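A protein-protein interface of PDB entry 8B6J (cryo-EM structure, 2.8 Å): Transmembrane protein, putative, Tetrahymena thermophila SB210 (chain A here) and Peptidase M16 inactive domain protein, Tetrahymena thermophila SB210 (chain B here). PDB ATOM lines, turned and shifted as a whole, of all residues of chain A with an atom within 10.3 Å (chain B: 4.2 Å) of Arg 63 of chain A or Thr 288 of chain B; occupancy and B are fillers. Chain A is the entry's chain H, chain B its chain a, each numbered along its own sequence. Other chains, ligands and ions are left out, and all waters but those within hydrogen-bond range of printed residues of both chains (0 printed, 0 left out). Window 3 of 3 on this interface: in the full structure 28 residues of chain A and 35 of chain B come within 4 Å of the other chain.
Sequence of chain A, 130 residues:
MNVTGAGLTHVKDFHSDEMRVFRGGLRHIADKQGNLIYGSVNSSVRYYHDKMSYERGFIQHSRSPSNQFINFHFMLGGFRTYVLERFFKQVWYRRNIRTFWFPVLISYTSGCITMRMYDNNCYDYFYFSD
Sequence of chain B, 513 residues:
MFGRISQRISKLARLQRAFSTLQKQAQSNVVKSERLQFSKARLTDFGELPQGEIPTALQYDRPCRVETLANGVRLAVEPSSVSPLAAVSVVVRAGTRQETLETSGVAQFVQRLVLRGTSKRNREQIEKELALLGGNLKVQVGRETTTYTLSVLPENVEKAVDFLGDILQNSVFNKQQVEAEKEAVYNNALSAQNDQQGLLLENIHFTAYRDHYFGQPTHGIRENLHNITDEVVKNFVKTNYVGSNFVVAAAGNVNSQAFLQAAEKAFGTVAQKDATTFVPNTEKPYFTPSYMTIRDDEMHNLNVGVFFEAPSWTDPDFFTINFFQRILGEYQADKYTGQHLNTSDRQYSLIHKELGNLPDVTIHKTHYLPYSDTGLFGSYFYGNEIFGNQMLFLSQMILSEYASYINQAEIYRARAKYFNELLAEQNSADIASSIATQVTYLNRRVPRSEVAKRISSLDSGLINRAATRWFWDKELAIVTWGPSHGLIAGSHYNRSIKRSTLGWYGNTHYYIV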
ATOM      1  N   GLN A  60     -13.335  -7.990   8.865  1.00  0.00           N
ATOM      2  CA  GLN A  60     -13.175  -6.546   8.795  1.00  0.00           C
ATOM      3  C   GLN A  60     -13.130  -6.106   7.339  1.00  0.00           C
ATOM      4  O   GLN A  60     -12.505  -6.762   6.503  1.00  0.00           O
ATOM      5  CB  GLN A  60     -11.901  -6.098   9.511  1.00  0.00           C
ATOM      6  CG  GLN A  60     -11.610  -4.614   9.387  1.00  0.00           C
ATOM      7  CD  GLN A  60     -10.421  -4.181  10.219  1.00  0.00           C
ATOM      8  OE1 GLN A  60      -9.512  -3.518   9.721  1.00  0.00           O
ATOM      9  NE2 GLN A  60     -10.425  -4.546  11.495  1.00  0.00           N
ATOM     10  N   HIS A  61     -13.796  -4.993   7.045  1.00  0.00           N
ATOM     11  CA  HIS A  61     -13.820  -4.412   5.710  1.00  0.00           C
ATOM     12  C   HIS A  61     -13.231  -3.013   5.764  1.00  0.00           C
ATOM     13  O   HIS A  61     -13.636  -2.198   6.599  1.00  0.00           O
ATOM     14  CB  HIS A  61     -15.243  -4.354   5.153  1.00  0.00           C
ATOM     15  CG  HIS A  61     -15.949  -5.673   5.154  1.00  0.00           C
ATOM     16  ND1 HIS A  61     -16.037  -6.470   4.035  1.00  0.00           N
ATOM     17  CD2 HIS A  61     -16.606  -6.331   6.138  1.00  0.00           C
ATOM     18  CE1 HIS A  61     -16.716  -7.564   4.329  1.00  0.00           C
ATOM     19  NE2 HIS A  61     -17.072  -7.504   5.599  1.00  0.00           N
ATOM     20  N   SER A  62     -12.278  -2.739   4.880  1.00  0.00           N
ATOM     21  CA  SER A  62     -11.699  -1.411   4.733  1.00  0.00           C
ATOM     22  C   SER A  62     -11.660  -1.069   3.253  1.00  0.00           C
ATOM     23  O   SER A  62     -11.221  -1.883   2.437  1.00  0.00           O
ATOM     24  CB  SER A  62     -10.296  -1.343   5.336  1.00  0.00           C
ATOM     25  OG  SER A  62      -9.419  -2.246   4.689  1.00  0.00           O
ATOM     26  N   ARG A  63     -12.115   0.131   2.914  1.00  0.00           N
ATOM     27  CA  ARG A  63     -12.220   0.567   1.533  1.00  0.00           C
ATOM     28  C   ARG A  63     -11.048   1.468   1.174  1.00  0.00           C
ATOM     29  O   ARG A  63     -10.469   2.139   2.032  1.00  0.00           O
ATOM     30  CB  ARG A  63     -13.539   1.307   1.302  1.00  0.00           C
ATOM     31  CG  ARG A  63     -13.847   1.608  -0.154  1.00  0.00           C
ATOM     32  CD  ARG A  63     -15.124   2.421  -0.291  1.00  0.00           C
ATOM     33  NE  ARG A  63     -16.258   1.783   0.367  1.00  0.00           N
ATOM     34  CZ  ARG A  63     -17.000   0.825  -0.173  1.00  0.00           C
ATOM     35  NH1 ARG A  63     -16.748   0.353  -1.383  1.00  0.00           N
ATOM     36  NH2 ARG A  63     -18.019   0.326   0.521  1.00  0.00           N
ATOM     37  N   SER A  64     -10.699   1.475  -0.106  1.00  0.00           N
ATOM     38  CA  SER A  64      -9.615   2.325  -0.566  1.00  0.00           C
ATOM     39  C   SER A  64      -9.985   3.792  -0.360  1.00  0.00           C
ATOM     40  O   SER A  64     -11.119   4.192  -0.649  1.00  0.00           O
ATOM     41  CB  SER A  64      -9.321   2.065  -2.043  1.00  0.00           C
ATOM     42  OG  SER A  64      -8.372   2.991  -2.542  1.00  0.00           O
ATOM     43  N   PRO A  65      -9.062   4.626   0.132  1.00  0.00           N
ATOM     44  CA  PRO A  65      -9.339   6.067   0.204  1.00  0.00           C
ATOM     45  C   PRO A  65      -9.553   6.725  -1.150  1.00  0.00           C
ATOM     46  O   PRO A  65      -9.836   7.927  -1.193  1.00  0.00           O
ATOM     47  CB  PRO A  65      -8.089   6.630   0.893  1.00  0.00           C
ATOM     48  CG  PRO A  65      -7.538   5.496   1.659  1.00  0.00           C
ATOM     49  CD  PRO A  65      -7.814   4.280   0.833  1.00  0.00           C
ATOM     50  N   SER A  66      -9.416   5.989  -2.254  1.00  0.00           N
ATOM     51  CA  SER A  66      -9.696   6.537  -3.573  1.00  0.00           C
ATOM     52  C   SER A  66     -11.179   6.524  -3.914  1.00  0.00           C
ATOM     53  O   SER A  66     -11.563   7.066  -4.956  1.00  0.00           O
ATOM     54  CB  SER A  66      -8.923   5.758  -4.638  1.00  0.00           C
ATOM     55  OG  SER A  66      -7.531   5.794  -4.384  1.00  0.00           O
ATOM     56  N   ASN A  67     -12.015   5.921  -3.074  1.00  0.00           N
ATOM     57  CA  ASN A  67     -13.459   5.892  -3.263  1.00  0.00           C
ATOM     58  C   ASN A  67     -14.169   6.446  -2.035  1.00  0.00           C
ATOM     59  O   ASN A  67     -15.242   5.980  -1.649  1.00  0.00           O
ATOM     60  CB  ASN A  67     -13.939   4.476  -3.564  1.00  0.00           C
ATOM     61  CG  ASN A  67     -13.199   3.847  -4.721  1.00  0.00           C
ATOM     62  OD1 ASN A  67     -12.701   2.727  -4.619  1.00  0.00           O
ATOM     63  ND2 ASN A  67     -13.116   4.569  -5.830  1.00  0.00           N
ATOM     64  N   GLN A  68     -13.568   7.454  -1.406  1.00  0.00           N
ATOM     65  CA  GLN A  68     -14.108   8.051  -0.197  1.00  0.00           C
ATOM     66  C   GLN A  68     -13.941   9.561  -0.267  1.00  0.00           C
ATOM     67  O   GLN A  68     -13.084  10.078  -0.987  1.00  0.00           O
ATOM     68  CB  GLN A  68     -13.416   7.495   1.055  1.00  0.00           C
ATOM     69  CG  GLN A  68     -13.567   5.992   1.222  1.00  0.00           C
ATOM     70  CD  GLN A  68     -12.891   5.472   2.471  1.00  0.00           C
ATOM     71  OE1 GLN A  68     -11.851   5.982   2.886  1.00  0.00           O
ATOM     72  NE2 GLN A  68     -13.484   4.457   3.085  1.00  0.00           N
ATOM     73  N   PHE A  69     -14.778  10.267   0.490  1.00  0.00           N
ATOM     74  CA  PHE A  69     -14.684  11.718   0.546  1.00  0.00           C
ATOM     75  C   PHE A  69     -13.293  12.140   1.001  1.00  0.00           C
ATOM     76  O   PHE A  69     -12.733  11.576   1.945  1.00  0.00           O
ATOM     77  CB  PHE A  69     -15.730  12.286   1.506  1.00  0.00           C
ATOM     78  CG  PHE A  69     -17.147  12.088   1.055  1.00  0.00           C
ATOM     79  CD1 PHE A  69     -17.771  13.031   0.259  1.00  0.00           C
ATOM     80  CD2 PHE A  69     -17.861  10.971   1.440  1.00  0.00           C
ATOM     81  CE1 PHE A  69     -19.075  12.856  -0.151  1.00  0.00           C
ATOM     82  CE2 PHE A  69     -19.165  10.791   1.033  1.00  0.00           C
ATOM     83  CZ  PHE A  69     -19.771  11.735   0.236  1.00  0.00           C
ATOM     84  N   THR B 207     -15.104  -9.148  -2.373  1.00  0.00           N
ATOM     85  CA  THR B 207     -14.519  -7.869  -1.987  1.00  0.00           C
ATOM     86  C   THR B 207     -14.271  -6.965  -3.187  1.00  0.00           C
ATOM     87  O   THR B 207     -14.293  -5.737  -3.047  1.00  0.00           O
ATOM     88  CB  THR B 207     -13.211  -8.092  -1.224  1.00  0.00           C
ATOM     89  OG1 THR B 207     -12.858  -6.899  -0.515  1.00  0.00           O
ATOM     90  CG2 THR B 207     -12.084  -8.449  -2.174  1.00  0.00           C
ATOM     91  N   ALA B 208     -14.030  -7.541  -4.366  1.00  0.00           N
ATOM     92  CA  ALA B 208     -13.755  -6.738  -5.548  1.00  0.00           C
ATOM     93  C   ALA B 208     -15.017  -6.112  -6.124  1.00  0.00           C
ATOM     94  O   ALA B 208     -14.964  -4.992  -6.644  1.00  0.00           O
ATOM     95  CB  ALA B 208     -13.068  -7.593  -6.613  1.00  0.00           C
ATOM     96  N   ARG B 210     -18.479  -5.212  -4.709  1.00  0.00           N
ATOM     97  CA  ARG B 210     -19.423  -5.065  -3.610  1.00  0.00           C
ATOM     98  C   ARG B 210     -20.740  -4.438  -4.039  1.00  0.00           C
ATOM     99  O   ARG B 210     -21.761  -4.663  -3.379  1.00  0.00           O
ATOM    100  CB  ARG B 210     -18.807  -4.219  -2.493  1.00  0.00           C
ATOM    101  CG  ARG B 210     -17.573  -4.829  -1.852  1.00  0.00           C
ATOM    102  CD  ARG B 210     -17.110  -3.999  -0.668  1.00  0.00           C
ATOM    103  NE  ARG B 210     -15.918  -4.551  -0.034  1.00  0.00           N
ATOM    104  CZ  ARG B 210     -15.926  -5.545   0.843  1.00  0.00           C
ATOM    105  NH1 ARG B 210     -17.050  -6.143   1.201  1.00  0.00           N
ATOM    106  NH2 ARG B 210     -14.775  -5.952   1.372  1.00  0.00           N
ATOM    107  N   TYR B 286     -18.350  -2.874 -11.760  1.00  0.00           N
ATOM    108  CA  TYR B 286     -17.191  -2.017 -11.549  1.00  0.00           C
ATOM    109  C   TYR B 286     -16.346  -2.517 -10.384  1.00  0.00           C
ATOM    110  O   TYR B 286     -16.865  -2.901  -9.332  1.00  0.00           O
ATOM    111  CB  TYR B 286     -17.638  -0.579 -11.301  1.00  0.00           C
ATOM    112  CG  TYR B 286     -18.238   0.071 -12.522  1.00  0.00           C
ATOM    113  CD1 TYR B 286     -17.434   0.710 -13.455  1.00  0.00           C
ATOM    114  CD2 TYR B 286     -19.606   0.038 -12.751  1.00  0.00           C
ATOM    115  CE1 TYR B 286     -17.975   1.300 -14.578  1.00  0.00           C
ATOM    116  CE2 TYR B 286     -20.157   0.627 -13.871  1.00  0.00           C
ATOM    117  CZ  TYR B 286     -19.335   1.257 -14.780  1.00  0.00           C
ATOM    118  OH  TYR B 286     -19.875   1.846 -15.898  1.00  0.00           O
ATOM    119  N   PHE B 287     -15.031  -2.508 -10.584  1.00  0.00           N
ATOM    120  CA  PHE B 287     -14.100  -3.003  -9.580  1.00  0.00           C
ATOM    121  C   PHE B 287     -14.125  -2.108  -8.347  1.00  0.00           C
ATOM    122  O   PHE B 287     -14.081  -0.879  -8.457  1.00  0.00           O
ATOM    123  CB  PHE B 287     -12.694  -3.061 -10.175  1.00  0.00           C
ATOM    124  CG  PHE B 287     -11.648  -3.573  -9.230  1.00  0.00           C
ATOM    125  CD1 PHE B 287     -11.634  -4.900  -8.844  1.00  0.00           C
ATOM    126  CD2 PHE B 287     -10.663  -2.731  -8.749  1.00  0.00           C
ATOM    127  CE1 PHE B 287     -10.667  -5.373  -7.982  1.00  0.00           C
ATOM    128  CE2 PHE B 287      -9.695  -3.198  -7.888  1.00  0.00           C
ATOM    129  CZ  PHE B 287      -9.696  -4.520  -7.505  1.00  0.00           C
ATOM    130  N   THR B 288     -14.192  -2.728  -7.171  1.00  0.00           N
ATOM    131  CA  THR B 288     -14.258  -2.008  -5.898  1.00  0.00           C
ATOM    132  C   THR B 288     -13.045  -2.364  -5.050  1.00  0.00           C
ATOM    133  O   THR B 288     -13.049  -3.399  -4.361  1.00  0.00           O
ATOM    134  CB  THR B 288     -15.547  -2.346  -5.151  1.00  0.00           C
ATOM    135  OG1 THR B 288     -16.678  -2.030  -5.971  1.00  0.00           O
ATOM    136  CG2 THR B 288     -15.636  -1.561  -3.853  1.00  0.00           C
ATOM    137  N   PRO B 289     -11.987  -1.552  -5.061  1.00  0.00           N
ATOM    138  CA  PRO B 289     -10.811  -1.872  -4.243  1.00  0.00           C
ATOM    139  C   PRO B 289     -11.172  -1.972  -2.769  1.00  0.00           C
ATOM    140  O   PRO B 289     -11.948  -1.171  -2.246  1.00  0.00           O
ATOM    141  CB  PRO B 289      -9.863  -0.698  -4.512  1.00  0.00           C
ATOM    142  CG  PRO B 289     -10.303  -0.144  -5.819  1.00  0.00           C
ATOM    143  CD  PRO B 289     -11.781  -0.341  -5.872  1.00  0.00           C
ATOM    144  N   SER B 290     -10.593  -2.963  -2.097  1.00  0.00           N
ATOM    145  CA  SER B 290     -10.907  -3.215  -0.698  1.00  0.00           C
ATOM    146  C   SER B 290      -9.849  -4.138  -0.111  1.00  0.00           C
ATOM    147  O   SER B 290      -9.017  -4.702  -0.827  1.00  0.00           O
ATOM    148  CB  SER B 290     -12.303  -3.824  -0.541  1.00  0.00           C
ATOM    149  OG  SER B 290     -13.308  -2.915  -0.952  1.00  0.00           O
ATOM    150  N   TYR B 493      -6.678  -0.173   4.422  1.00  0.00           N
ATOM    151  CA  TYR B 493      -6.114   0.285   3.155  1.00  0.00           C
ATOM    152  C   TYR B 493      -5.394   1.603   3.404  1.00  0.00           C
ATOM    153  O   TYR B 493      -6.020   2.662   3.479  1.00  0.00           O
ATOM    154  CB  TYR B 493      -7.217   0.440   2.116  1.00  0.00           C
ATOM    155  CG  TYR B 493      -6.756   0.277   0.688  1.00  0.00           C
ATOM    156  CD1 TYR B 493      -5.991   1.251   0.068  1.00  0.00           C
ATOM    157  CD2 TYR B 493      -7.098  -0.850  -0.044  1.00  0.00           C
ATOM    158  CE1 TYR B 493      -5.572   1.105  -1.237  1.00  0.00           C
ATOM    159  CE2 TYR B 493      -6.684  -1.005  -1.349  1.00  0.00           C
ATOM    160  CZ  TYR B 493      -5.922  -0.026  -1.941  1.00  0.00           C
ATOM    161  OH  TYR B 493      -5.508  -0.176  -3.242  1.00  0.00           O
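A ring nitrogen (ND1) of His 61 of chain A lies within hydrogen-bond range of the guanidinium group (NH2) of Arg 210 of chain B. OG of Ser 62 of chain A is in hydrogen-bond range of N of Tyr 493 of chain B (3.4 Å).
The side-chain hydroxyl (OG1) of Thr 207 of chain B lies within hydrogen-bond range of the guanidinium group (NH2) of Arg 210 of chain B, 2.9 Å away. O of Ala 208 of chain B lies within hydrogen-bond range of N of Thr 288 of chain B (2.4 Å). The guanidinium group of Arg 210 of chain B sits at hydrogen-bond distance from the side-chain hydroxyl of Ser 290 of chain B, 3.2 Å away. O of Tyr 286 of chain B lies within hydrogen-bond range of OG1 of Thr 288 of chain B, 3.5 Å away. O of Thr 288 of chain B is in hydrogen-bond range of OG of Ser 290 of chain B, at 3.5 Å. The backbone NH of Ser 66 of chain A sits close to the side-chain hydroxyl of Ser 64 of chain A (3.2 Å).
Among the printed residues, pairs that only touch across the chains: Ser 62 of chain A with Ser 290 of chain B (3.4 Å), Arg 63 of chain A with Thr 288 of chain B (3.3 Å), Arg 63 of chain A with Pro 289 of chain B (3.96 Å), Arg 63 of chain A with Tyr 493 of chain B (3.7 Å), Ser 64 of chain A with Pro 289 of chain B (3.6 Å), Ser 64 of chain A with Tyr 493 of chain B (3.6 Å), Pro 65 of chain A with Tyr 493 of chain B (3.6 Å) and Asn 67 of chain A with Pro 289 of chain B (3.4 Å).
Printed residues of chain B within 4 Å of His 61 of chain A: Arg 210. Of chain B, only Thr 288 (3.3 Å), Pro 289 (3.96 Å) and Tyr 493 (3.7 Å) come within 4 Å of Arg 63 of chain A. Of the printed residues of chain B, Ser 64 of chain A touches Pro 289 (3.6 Å) and Tyr 493 (3.6 Å). Printed residues of chain B within 4 Å of Asn 67 of chain A: Pro 289. Of the printed residues of chain A, Arg 210 of chain B touches His 61 (3.0 Å). No residue of chain A comes within 4 Å of Phe 287 of chain B. Of the printed residues of chain A, Thr 288 of chain B touches Arg 63. Of chain A, only Ser 62 (3.4 Å) comes within 4 Å of Ser 290 of chain B. Printed residues of chain A within 4 Å of Tyr 493 of chain B: Ser 62, Arg 63, Ser 64 and Pro 65. The nearest printed residue of chain B that does not touch Arg 63 of chain A is Ser 290 of chain B (4.4 Å). The nearest residue of chain A that does not touch Thr 288 of chain B is Asn 67 of chain A (5.1 Å). The nearest printed residue of chain A that does not touch Arg 210 of chain B is Arg 63 of chain A (4.4 Å).
Among the printed residues, 10 pairs touch across the chains. Among the printed residues, no Asp or Glu carboxylate lies within 4 Å of a Lys or Arg side-chain nitrogen of the other chain.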
